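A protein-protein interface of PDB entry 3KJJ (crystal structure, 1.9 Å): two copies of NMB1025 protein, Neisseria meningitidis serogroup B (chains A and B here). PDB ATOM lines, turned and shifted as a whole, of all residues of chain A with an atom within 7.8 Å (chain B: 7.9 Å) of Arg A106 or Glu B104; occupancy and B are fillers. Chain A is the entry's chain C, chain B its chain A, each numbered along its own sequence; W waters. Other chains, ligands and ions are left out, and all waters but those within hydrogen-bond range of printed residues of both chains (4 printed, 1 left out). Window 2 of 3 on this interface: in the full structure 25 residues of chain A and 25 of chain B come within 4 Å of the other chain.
Of the printed residues of chain B, Tyr A74 touches Val B103 (3.6 Å).
Of the printed residues of chain B, Arg A106 touches Met B78, Val B103 and Glu B104.
Of the printed residues of chain A, Ala B101 touches Glu A115.
Printed residues of chain A within 4 Å of Glu B104: Ala A105 and Arg A106.
The side-chain sulfur (SG) of Cys B102 lies close to the backbone carbonyl oxygen (O) of Ile B73 (3.8 Å).
The backbone NH (N) of Met B78 sits at hydrogen-bond distance from the side-chain carboxylate (OE2) of Glu B104 (2.9 Å).
N of Ile B73 is in hydrogen-bond range of O of Ala B101 (2.8 Å).
The backbone NH (N) of Tyr A74 sits at hydrogen-bond distance from the backbone carbonyl oxygen (O) of Glu A115 (2.9 Å).
The backbone carbonyl oxygen (O) of Ile B73 sits at hydrogen-bond distance from the backbone NH (N) of Val B103 (2.9 Å).
The backbone NH (N) of Leu B75 lies within hydrogen-bond range of the backbone carbonyl oxygen (O) of Val B103, at 3.0 Å.
OE1 of Glu B104 lies within salt-bridge range of NH1 of Arg A106, at 2.8 Å.
Water W4 lies within hydrogen-bond range of OE2 of Glu A115 (2.6 Å) and N of Cys B102 (2.9 Å).
Water W1 lies within hydrogen-bond range of the backbone NH (N) of Ala A108 (2.7 Å), the backbone carbonyl oxygen (O) of Cys B102 (2.8 Å) and the side-chain carboxylate (OE1) of Glu A115 (2.8 Å).
Water W2 lies within hydrogen-bond range of O of Glu B104 (2.8 Å) and O of Glu A104 (2.9 Å).
Water W3 bridges the backbone carbonyl oxygen of Glu B104 (3.1 Å) and the backbone NH of Arg A106 (3.2 Å).
Ala A105 touches Glu B104, but with the chains exchanged Glu A104 does not touch Ala B105 (6.1 Å).
Arg A106 touches Val B103, but with the chains exchanged Val A103 does not touch Arg B106 (10.3 Å).
Arg A106 touches Glu B104, but with the chains exchanged Glu A104 does not touch Arg B106 (7.8 Å).
Leu A107 touches Val B103, but with the chains exchanged Val A103 does not touch Leu B107 (11.8 Å).
9 positions are printed for both chains.
Of the 11 pairs that touch across the chains among the printed residues, none has its exchanged pair printed and touching as well.
Val B103 touches Tyr A74 (CG1 to CG, 3.6 Å).
Ala A105 touches Val B103 (CB to CB, 3.9 Å).
CB of Ala A105 touches O of Glu B104, 3.3 Å away.
Arg A106 touches Met B78.
Val B103 touches Arg A106.
Leu A107 touches Met B78 (O to CG, 3.4 Å).
CD2 of Leu A107 touches CG1 of Val B103, 3.7 Å away.
Ala A108 touches Met B78.
CB of Ala B101 touches OE2 of Glu A115 (3.4 Å).
Glu A115 touches Cys B102 (OE1 to O, 3.9 Å).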
ATOM      1  N   TYR A  74      25.550 -13.364 -10.540  1.00  0.00           N
ATOM      2  CA  TYR A  74      24.394 -14.191 -10.886  1.00  0.00           C
ATOM      3  C   TYR A  74      23.482 -13.314 -11.726  1.00  0.00           C
ATOM      4  O   TYR A  74      23.192 -12.181 -11.340  1.00  0.00           O
ATOM      5  CB  TYR A  74      23.650 -14.696  -9.633  1.00  0.00           C
ATOM      6  CG  TYR A  74      24.520 -15.378  -8.583  1.00  0.00           C
ATOM      7  CD1 TYR A  74      24.813 -16.742  -8.660  1.00  0.00           C
ATOM      8  CD2 TYR A  74      25.028 -14.657  -7.502  1.00  0.00           C
ATOM      9  CE1 TYR A  74      25.611 -17.374  -7.684  1.00  0.00           C
ATOM     10  CE2 TYR A  74      25.819 -15.272  -6.526  1.00  0.00           C
ATOM     11  CZ  TYR A  74      26.106 -16.621  -6.619  1.00  0.00           C
ATOM     12  OH  TYR A  74      26.897 -17.212  -5.653  1.00  0.00           O
ATOM     13  N   LEU A  75      23.062 -13.830 -12.879  1.00  0.00           N
ATOM     14  CA  LEU A  75      22.090 -13.153 -13.744  1.00  0.00           C
ATOM     15  C   LEU A  75      20.827 -13.988 -13.766  1.00  0.00           C
ATOM     16  O   LEU A  75      20.906 -15.205 -13.854  1.00  0.00           O
ATOM     17  CB  LEU A  75      22.632 -13.028 -15.174  1.00  0.00           C
ATOM     18  CG  LEU A  75      23.781 -12.042 -15.396  1.00  0.00           C
ATOM     19  CD1 LEU A  75      24.455 -12.307 -16.739  1.00  0.00           C
ATOM     20  CD2 LEU A  75      23.291 -10.606 -15.273  1.00  0.00           C
ATOM     21  N   ARG A  76      19.665 -13.338 -13.664  1.00  0.00           N
ATOM     22  CA  ARG A  76      18.381 -14.033 -13.760  1.00  0.00           C
ATOM     23  C   ARG A  76      18.319 -14.803 -15.085  1.00  0.00           C
ATOM     24  O   ARG A  76      17.851 -15.947 -15.145  1.00  0.00           O
ATOM     25  CB  ARG A  76      17.223 -13.021 -13.659  1.00  0.00           C
ATOM     26  CG  ARG A  76      15.824 -13.631 -13.839  1.00  0.00           C
ATOM     27  CD  ARG A  76      14.707 -12.616 -13.599  1.00  0.00           C
ATOM     28  NE  ARG A  76      13.382 -13.229 -13.733  1.00  0.00           N
ATOM     29  CZ  ARG A  76      12.752 -13.907 -12.774  1.00  0.00           C
ATOM     30  NH1 ARG A  76      13.299 -14.077 -11.564  1.00  0.00           N
ATOM     31  NH2 ARG A  76      11.556 -14.421 -13.026  1.00  0.00           N
ATOM     32  N   ASP A  77      18.858 -14.178 -16.128  1.00  0.00           N
ATOM     33  CA  ASP A  77      18.717 -14.642 -17.503  1.00  0.00           C
ATOM     34  C   ASP A  77      20.037 -14.415 -18.246  1.00  0.00           C
ATOM     35  O   ASP A  77      20.442 -13.276 -18.468  1.00  0.00           O
ATOM     36  CB  ASP A  77      17.561 -13.859 -18.153  1.00  0.00           C
ATOM     37  CG  ASP A  77      17.211 -14.344 -19.558  1.00  0.00           C
ATOM     38  OD1 ASP A  77      16.011 -14.398 -19.882  1.00  0.00           O
ATOM     39  OD2 ASP A  77      18.121 -14.649 -20.343  1.00  0.00           O
ATOM     40  N   VAL A 103      27.127 -16.888 -13.567  1.00  0.00           N
ATOM     41  CA  VAL A 103      26.195 -18.000 -13.767  1.00  0.00           C
ATOM     42  C   VAL A 103      24.748 -17.529 -13.736  1.00  0.00           C
ATOM     43  O   VAL A 103      24.438 -16.463 -13.196  1.00  0.00           O
ATOM     44  CB  VAL A 103      26.407 -19.152 -12.747  1.00  0.00           C
ATOM     45  CG1 VAL A 103      27.828 -19.754 -12.880  1.00  0.00           C
ATOM     46  CG2 VAL A 103      26.129 -18.677 -11.324  1.00  0.00           C
ATOM     47  N   GLU A 104      23.874 -18.320 -14.341  1.00  0.00           N
ATOM     48  CA  GLU A 104      22.472 -17.996 -14.366  1.00  0.00           C
ATOM     49  C   GLU A 104      21.773 -18.584 -13.151  1.00  0.00           C
ATOM     50  O   GLU A 104      21.806 -19.801 -12.933  1.00  0.00           O
ATOM     51  CB  GLU A 104      21.826 -18.520 -15.643  1.00  0.00           C
ATOM     52  CG  GLU A 104      20.481 -17.881 -15.918  1.00  0.00           C
ATOM     53  CD  GLU A 104      19.733 -18.615 -16.986  1.00  0.00           C
ATOM     54  OE1 GLU A 104      19.098 -19.630 -16.655  1.00  0.00           O
ATOM     55  OE2 GLU A 104      19.789 -18.178 -18.155  1.00  0.00           O
ATOM     56  N   ALA A 105      21.169 -17.704 -12.356  1.00  0.00           N
ATOM     57  CA  ALA A 105      20.335 -18.103 -11.221  1.00  0.00           C
ATOM     58  C   ALA A 105      19.259 -17.061 -10.953  1.00  0.00           C
ATOM     59  O   ALA A 105      19.550 -15.861 -10.954  1.00  0.00           O
ATOM     60  CB  ALA A 105      21.189 -18.312  -9.974  1.00  0.00           C
ATOM     61  N   ARG A 106      18.027 -17.517 -10.704  1.00  0.00           N
ATOM     62  CA  ARG A 106      16.931 -16.612 -10.338  1.00  0.00           C
ATOM     63  C   ARG A 106      17.187 -16.039  -8.943  1.00  0.00           C
ATOM     64  O   ARG A 106      17.689 -16.734  -8.060  1.00  0.00           O
ATOM     65  CB  ARG A 106      15.574 -17.333 -10.367  1.00  0.00           C
ATOM     66  CG  ARG A 106      14.964 -17.552 -11.759  1.00  0.00           C
ATOM     67  CD  ARG A 106      13.826 -18.547 -11.646  1.00  0.00           C
ATOM     68  NE  ARG A 106      13.265 -18.988 -12.926  1.00  0.00           N
ATOM     69  CZ  ARG A 106      12.966 -20.256 -13.214  1.00  0.00           C
ATOM     70  NH1 ARG A 106      13.220 -21.219 -12.336  1.00  0.00           N
ATOM     71  NH2 ARG A 106      12.442 -20.576 -14.392  1.00  0.00           N
ATOM     72  N   LEU A 107      16.826 -14.773  -8.752  1.00  0.00           N
ATOM     73  CA  LEU A 107      17.101 -14.061  -7.505  1.00  0.00           C
ATOM     74  C   LEU A 107      15.842 -13.914  -6.659  1.00  0.00           C
ATOM     75  O   LEU A 107      14.774 -14.373  -7.056  1.00  0.00           O
ATOM     76  CB  LEU A 107      17.730 -12.705  -7.830  1.00  0.00           C
ATOM     77  CG  LEU A 107      18.899 -12.878  -8.810  1.00  0.00           C
ATOM     78  CD1 LEU A 107      19.333 -11.555  -9.421  1.00  0.00           C
ATOM     79  CD2 LEU A 107      20.074 -13.615  -8.161  1.00  0.00           C
ATOM     80  N   ALA A 108      15.962 -13.278  -5.496  1.00  0.00           N
ATOM     81  CA  ALA A 108      14.842 -13.205  -4.553  1.00  0.00           C
ATOM     82  C   ALA A 108      13.581 -12.539  -5.122  1.00  0.00           C
ATOM     83  O   ALA A 108      12.465 -12.958  -4.813  1.00  0.00           O
ATOM     84  CB  ALA A 108      15.267 -12.544  -3.252  1.00  0.00           C
ATOM     85  N   ARG A 109      13.761 -11.513  -5.948  1.00  0.00           N
ATOM     86  CA  ARG A 109      12.628 -10.819  -6.569  1.00  0.00           C
ATOM     87  C   ARG A 109      12.671 -10.992  -8.083  1.00  0.00           C
ATOM     88  O   ARG A 109      13.750 -10.960  -8.674  1.00  0.00           O
ATOM     89  CB  ARG A 109      12.625  -9.334  -6.195  1.00  0.00           C
ATOM     90  CG  ARG A 109      12.925  -9.080  -4.730  1.00  0.00           C
ATOM     91  CD  ARG A 109      11.736  -8.586  -3.943  1.00  0.00           C
ATOM     92  NE  ARG A 109      12.165  -8.044  -2.652  1.00  0.00           N
ATOM     93  CZ  ARG A 109      12.573  -6.792  -2.442  1.00  0.00           C
ATOM     94  NH1 ARG A 109      12.606  -5.910  -3.437  1.00  0.00           N
ATOM     95  NH2 ARG A 109      12.950  -6.418  -1.227  1.00  0.00           N
ATOM     96  N   PRO A 110      11.493 -11.179  -8.718  1.00  0.00           N
ATOM     97  CA  PRO A 110      11.463 -11.461 -10.160  1.00  0.00           C
ATOM     98  C   PRO A 110      12.029 -10.338 -11.032  1.00  0.00           C
ATOM     99  O   PRO A 110      12.600 -10.623 -12.086  1.00  0.00           O
ATOM    100  CB  PRO A 110       9.975 -11.703 -10.462  1.00  0.00           C
ATOM    101  CG  PRO A 110       9.226 -11.283  -9.240  1.00  0.00           C
ATOM    102  CD  PRO A 110      10.175 -11.344  -8.084  1.00  0.00           C
ATOM    103  N   TRP A 112      14.561  -8.436 -10.301  1.00  0.00           N
ATOM    104  CA  TRP A 112      16.019  -8.347 -10.136  1.00  0.00           C
ATOM    105  C   TRP A 112      16.739  -9.156 -11.213  1.00  0.00           C
ATOM    106  O   TRP A 112      16.531 -10.361 -11.329  1.00  0.00           O
ATOM    107  CB  TRP A 112      16.443  -8.833  -8.743  1.00  0.00           C
ATOM    108  CG  TRP A 112      16.035  -7.920  -7.589  1.00  0.00           C
ATOM    109  CD1 TRP A 112      15.534  -6.645  -7.679  1.00  0.00           C
ATOM    110  CD2 TRP A 112      16.159  -8.201  -6.189  1.00  0.00           C
ATOM    111  NE1 TRP A 112      15.310  -6.134  -6.421  1.00  0.00           N
ATOM    112  CE2 TRP A 112      15.688  -7.067  -5.489  1.00  0.00           C
ATOM    113  CE3 TRP A 112      16.606  -9.312  -5.457  1.00  0.00           C
ATOM    114  CZ2 TRP A 112      15.659  -7.008  -4.094  1.00  0.00           C
ATOM    115  CZ3 TRP A 112      16.577  -9.253  -4.068  1.00  0.00           C
ATOM    116  CH2 TRP A 112      16.107  -8.111  -3.402  1.00  0.00           C
ATOM    117  N   GLU A 115      22.755  -9.980  -9.418  1.00  0.00           N
ATOM    118  CA  GLU A 115      23.264  -9.918  -8.057  1.00  0.00           C
ATOM    119  C   GLU A 115      24.764 -10.188  -8.106  1.00  0.00           C
ATOM    120  O   GLU A 115      25.204 -11.099  -8.803  1.00  0.00           O
ATOM    121  CB  GLU A 115      22.549 -10.936  -7.157  1.00  0.00           C
ATOM    122  CG  GLU A 115      23.043 -10.956  -5.711  1.00  0.00           C
ATOM    123  CD  GLU A 115      22.143 -11.725  -4.762  1.00  0.00           C
ATOM    124  OE1 GLU A 115      21.048 -12.155  -5.172  1.00  0.00           O
ATOM    125  OE2 GLU A 115      22.521 -11.885  -3.584  1.00  0.00           O
ATOM    126  N   ILE B  73      23.269 -19.239   0.145  1.00  0.00           N
ATOM    127  CA  ILE B  73      22.115 -20.111   0.267  1.00  0.00           C
ATOM    128  C   ILE B  73      21.566 -20.366  -1.118  1.00  0.00           C
ATOM    129  O   ILE B  73      21.238 -19.427  -1.843  1.00  0.00           O
ATOM    130  CB  ILE B  73      21.013 -19.506   1.172  1.00  0.00           C
ATOM    131  CG1 ILE B  73      21.582 -19.131   2.542  1.00  0.00           C
ATOM    132  CG2 ILE B  73      19.836 -20.495   1.321  1.00  0.00           C
ATOM    133  CD1 ILE B  73      20.763 -18.085   3.266  1.00  0.00           C
ATOM    134  N   TYR B  74      21.516 -21.647  -1.483  1.00  0.00           N
ATOM    135  CA  TYR B  74      20.945 -22.080  -2.742  1.00  0.00           C
ATOM    136  C   TYR B  74      19.607 -22.724  -2.411  1.00  0.00           C
ATOM    137  O   TYR B  74      19.535 -23.617  -1.561  1.00  0.00           O
ATOM    138  CB  TYR B  74      21.866 -23.106  -3.434  1.00  0.00           C
ATOM    139  CG  TYR B  74      23.278 -22.619  -3.726  1.00  0.00           C
ATOM    140  CD1 TYR B  74      23.547 -21.805  -4.826  1.00  0.00           C
ATOM    141  CD2 TYR B  74      24.344 -22.983  -2.906  1.00  0.00           C
ATOM    142  CE1 TYR B  74      24.834 -21.361  -5.101  1.00  0.00           C
ATOM    143  CE2 TYR B  74      25.640 -22.543  -3.172  1.00  0.00           C
ATOM    144  CZ  TYR B  74      25.877 -21.733  -4.266  1.00  0.00           C
ATOM    145  OH  TYR B  74      27.156 -21.293  -4.526  1.00  0.00           O
ATOM    146  N   LEU B  75      18.547 -22.257  -3.054  1.00  0.00           N
ATOM    147  CA  LEU B  75      17.242 -22.899  -2.934  1.00  0.00           C
ATOM    148  C   LEU B  75      16.900 -23.544  -4.252  1.00  0.00           C
ATOM    149  O   LEU B  75      17.231 -23.011  -5.312  1.00  0.00           O
ATOM    150  CB  LEU B  75      16.152 -21.883  -2.577  1.00  0.00           C
ATOM    151  CG  LEU B  75      16.212 -21.107  -1.261  1.00  0.00           C
ATOM    152  CD1 LEU B  75      15.215 -19.954  -1.296  1.00  0.00           C
ATOM    153  CD2 LEU B  75      15.930 -22.018  -0.074  1.00  0.00           C
ATOM    154  N   ARG B  76      16.244 -24.698  -4.194  1.00  0.00           N
ATOM    155  CA  ARG B  76      15.732 -25.328  -5.410  1.00  0.00           C
ATOM    156  C   ARG B  76      14.668 -24.417  -6.027  1.00  0.00           C
ATOM    157  O   ARG B  76      14.589 -24.260  -7.248  1.00  0.00           O
ATOM    158  CB  ARG B  76      15.138 -26.698  -5.076  1.00  0.00           C
ATOM    159  CG  ARG B  76      14.699 -27.515  -6.282  1.00  0.00           C
ATOM    160  CD  ARG B  76      14.018 -28.809  -5.836  1.00  0.00           C
ATOM    161  NE  ARG B  76      13.359 -29.511  -6.945  1.00  0.00           N
ATOM    162  CZ  ARG B  76      13.986 -30.195  -7.897  1.00  0.00           C
ATOM    163  NH1 ARG B  76      15.319 -30.289  -7.903  1.00  0.00           N
ATOM    164  NH2 ARG B  76      13.273 -30.793  -8.849  1.00  0.00           N
ATOM    165  N   ASP B  77      13.881 -23.793  -5.160  1.00  0.00           N
ATOM    166  CA  ASP B  77      12.728 -23.019  -5.574  1.00  0.00           C
ATOM    167  C   ASP B  77      12.671 -21.757  -4.734  1.00  0.00           C
ATOM    168  O   ASP B  77      12.489 -21.839  -3.511  1.00  0.00           O
ATOM    169  CB  ASP B  77      11.464 -23.869  -5.376  1.00  0.00           C
ATOM    170  CG  ASP B  77      10.231 -23.247  -6.003  1.00  0.00           C
ATOM    171  OD1 ASP B  77       9.375 -24.013  -6.487  1.00  0.00           O
ATOM    172  OD2 ASP B  77      10.115 -22.003  -6.018  1.00  0.00           O
ATOM    173  N   MET B  78      12.834 -20.600  -5.387  1.00  0.00           N
ATOM    174  CA  MET B  78      12.829 -19.292  -4.715  1.00  0.00           C
ATOM    175  C   MET B  78      11.476 -18.985  -4.056  1.00  0.00           C
ATOM    176  O   MET B  78      11.349 -18.021  -3.307  1.00  0.00           O
ATOM    177  CB  MET B  78      13.286 -18.164  -5.672  1.00  0.00           C
ATOM    178  CG  MET B  78      13.539 -16.775  -5.007  1.00  0.00           C
ATOM    179  SD  MET B  78      14.952 -16.697  -3.586  1.00  0.00           S
ATOM    180  CE  MET B  78      16.366 -17.501  -4.644  1.00  0.00           C
ATOM    181  N   GLY B  79      10.473 -19.822  -4.314  1.00  0.00           N
ATOM    182  CA  GLY B  79       9.192 -19.738  -3.595  1.00  0.00           C
ATOM    183  C   GLY B  79       9.302 -20.172  -2.141  1.00  0.00           C
ATOM    184  O   GLY B  79       8.411 -19.915  -1.336  1.00  0.00           O
ATOM    185  N   ASP B  80      10.403 -20.834  -1.792  1.00  0.00           N
ATOM    186  CA  ASP B  80      10.642 -21.217  -0.407  1.00  0.00           C
ATOM    187  C   ASP B  80      11.396 -20.132   0.357  1.00  0.00           C
ATOM    188  O   ASP B  80      11.796 -20.352   1.503  1.00  0.00           O
ATOM    189  CB  ASP B  80      11.396 -22.554  -0.320  1.00  0.00           C
ATOM    190  CG  ASP B  80      10.555 -23.739  -0.768  1.00  0.00           C
ATOM    191  OD1 ASP B  80       9.338 -23.748  -0.503  1.00  0.00           O
ATOM    192  OD2 ASP B  80      11.117 -24.682  -1.369  1.00  0.00           O
ATOM    193  N   ALA B 101      24.167 -14.225   0.581  1.00  0.00           N
ATOM    194  CA  ALA B 101      23.492 -14.181  -0.714  1.00  0.00           C
ATOM    195  C   ALA B 101      22.605 -15.408  -0.848  1.00  0.00           C
ATOM    196  O   ALA B 101      22.972 -16.505  -0.418  1.00  0.00           O
ATOM    197  CB  ALA B 101      24.494 -14.112  -1.852  1.00  0.00           C
ATOM    198  N   CYS B 102      21.434 -15.215  -1.451  1.00  0.00           N
ATOM    199  CA  CYS B 102      20.507 -16.304  -1.670  1.00  0.00           C
ATOM    200  C   CYS B 102      20.082 -16.359  -3.129  1.00  0.00           C
ATOM    201  O   CYS B 102      19.478 -15.416  -3.631  1.00  0.00           O
ATOM    202  CB  CYS B 102      19.273 -16.145  -0.773  1.00  0.00           C
ATOM    203  SG  CYS B 102      18.101 -17.470  -1.039  1.00  0.00           S
ATOM    204  N   VAL B 103      20.407 -17.465  -3.800  1.00  0.00           N
ATOM    205  CA  VAL B 103      20.089 -17.640  -5.227  1.00  0.00           C
ATOM    206  C   VAL B 103      19.342 -18.936  -5.492  1.00  0.00           C
ATOM    207  O   VAL B 103      19.436 -19.881  -4.703  1.00  0.00           O
ATOM    208  CB  VAL B 103      21.349 -17.579  -6.141  1.00  0.00           C
ATOM    209  CG1 VAL B 103      21.903 -16.149  -6.232  1.00  0.00           C
ATOM    210  CG2 VAL B 103      22.427 -18.563  -5.675  1.00  0.00           C
ATOM    211  N   GLU B 104      18.600 -18.975  -6.600  1.00  0.00           N
ATOM    212  CA  GLU B 104      17.881 -20.182  -6.997  1.00  0.00           C
ATOM    213  C   GLU B 104      18.752 -21.107  -7.857  1.00  0.00           C
ATOM    214  O   GLU B 104      19.176 -20.742  -8.960  1.00  0.00           O
ATOM    215  CB  GLU B 104      16.572 -19.837  -7.737  1.00  0.00           C
ATOM    216  CG  GLU B 104      15.568 -20.992  -7.775  1.00  0.00           C
ATOM    217  CD  GLU B 104      14.428 -20.730  -8.736  1.00  0.00           C
ATOM    218  OE1 GLU B 104      14.635 -20.907  -9.951  1.00  0.00           O
ATOM    219  OE2 GLU B 104      13.331 -20.351  -8.275  1.00  0.00           O
ATOM    220  N   ALA B 105      19.025 -22.295  -7.331  1.00  0.00           N
ATOM    221  CA  ALA B 105      19.700 -23.354  -8.087  1.00  0.00           C
ATOM    222  C   ALA B 105      19.257 -24.730  -7.618  1.00  0.00           C
ATOM    223  O   ALA B 105      19.125 -24.979  -6.421  1.00  0.00           O
ATOM    224  CB  ALA B 105      21.216 -23.225  -7.965  1.00  0.00           C
ATOM    225  N   ARG B 106      19.051 -25.632  -8.572  1.00  0.00           N
ATOM    226  CA  ARG B 106      18.766 -27.024  -8.258  1.00  0.00           C
ATOM    227  C   ARG B 106      19.978 -27.756  -7.691  1.00  0.00           C
ATOM    228  O   ARG B 106      21.118 -27.447  -8.032  1.00  0.00           O
ATOM    229  CB  ARG B 106      18.264 -27.735  -9.503  1.00  0.00           C
ATOM    230  CG  ARG B 106      16.936 -27.201  -9.924  1.00  0.00           C
ATOM    231  CD  ARG B 106      16.243 -28.165 -10.807  1.00  0.00           C
ATOM    232  NE  ARG B 106      14.820 -27.886 -10.848  1.00  0.00           N
ATOM    233  CZ  ARG B 106      13.935 -28.696 -11.414  1.00  0.00           C
ATOM    234  NH1 ARG B 106      14.351 -29.820 -11.985  1.00  0.00           N
ATOM    235  NH2 ARG B 106      12.647 -28.382 -11.407  1.00  0.00           N
ATOM    236  N   LEU B 107      19.715 -28.727  -6.824  1.00  0.00           N
ATOM    237  CA  LEU B 107      20.777 -29.421  -6.089  1.00  0.00           C
ATOM    238  C   LEU B 107      20.894 -30.864  -6.567  1.00  0.00           C
ATOM    239  O   LEU B 107      20.138 -31.278  -7.462  1.00  0.00           O
ATOM    240  CB  LEU B 107      20.527 -29.305  -4.579  1.00  0.00           C
ATOM    241  CG  LEU B 107      20.216 -27.852  -4.178  1.00  0.00           C
ATOM    242  CD1 LEU B 107      19.655 -27.753  -2.782  1.00  0.00           C
ATOM    243  CD2 LEU B 107      21.415 -26.910  -4.359  1.00  0.00           C
HETATM  244  O   HOH W   1      18.467 -12.944  -4.448  1.00  0.00           O
HETATM  245  O   HOH W   2      20.220 -21.703 -11.405  1.00  0.00           O
HETATM  246  O   HOH W   3      17.554 -20.524 -11.537  1.00  0.00           O
HETATM  247  O   HOH W   4      20.700 -12.423  -1.786  1.00  0.00           O
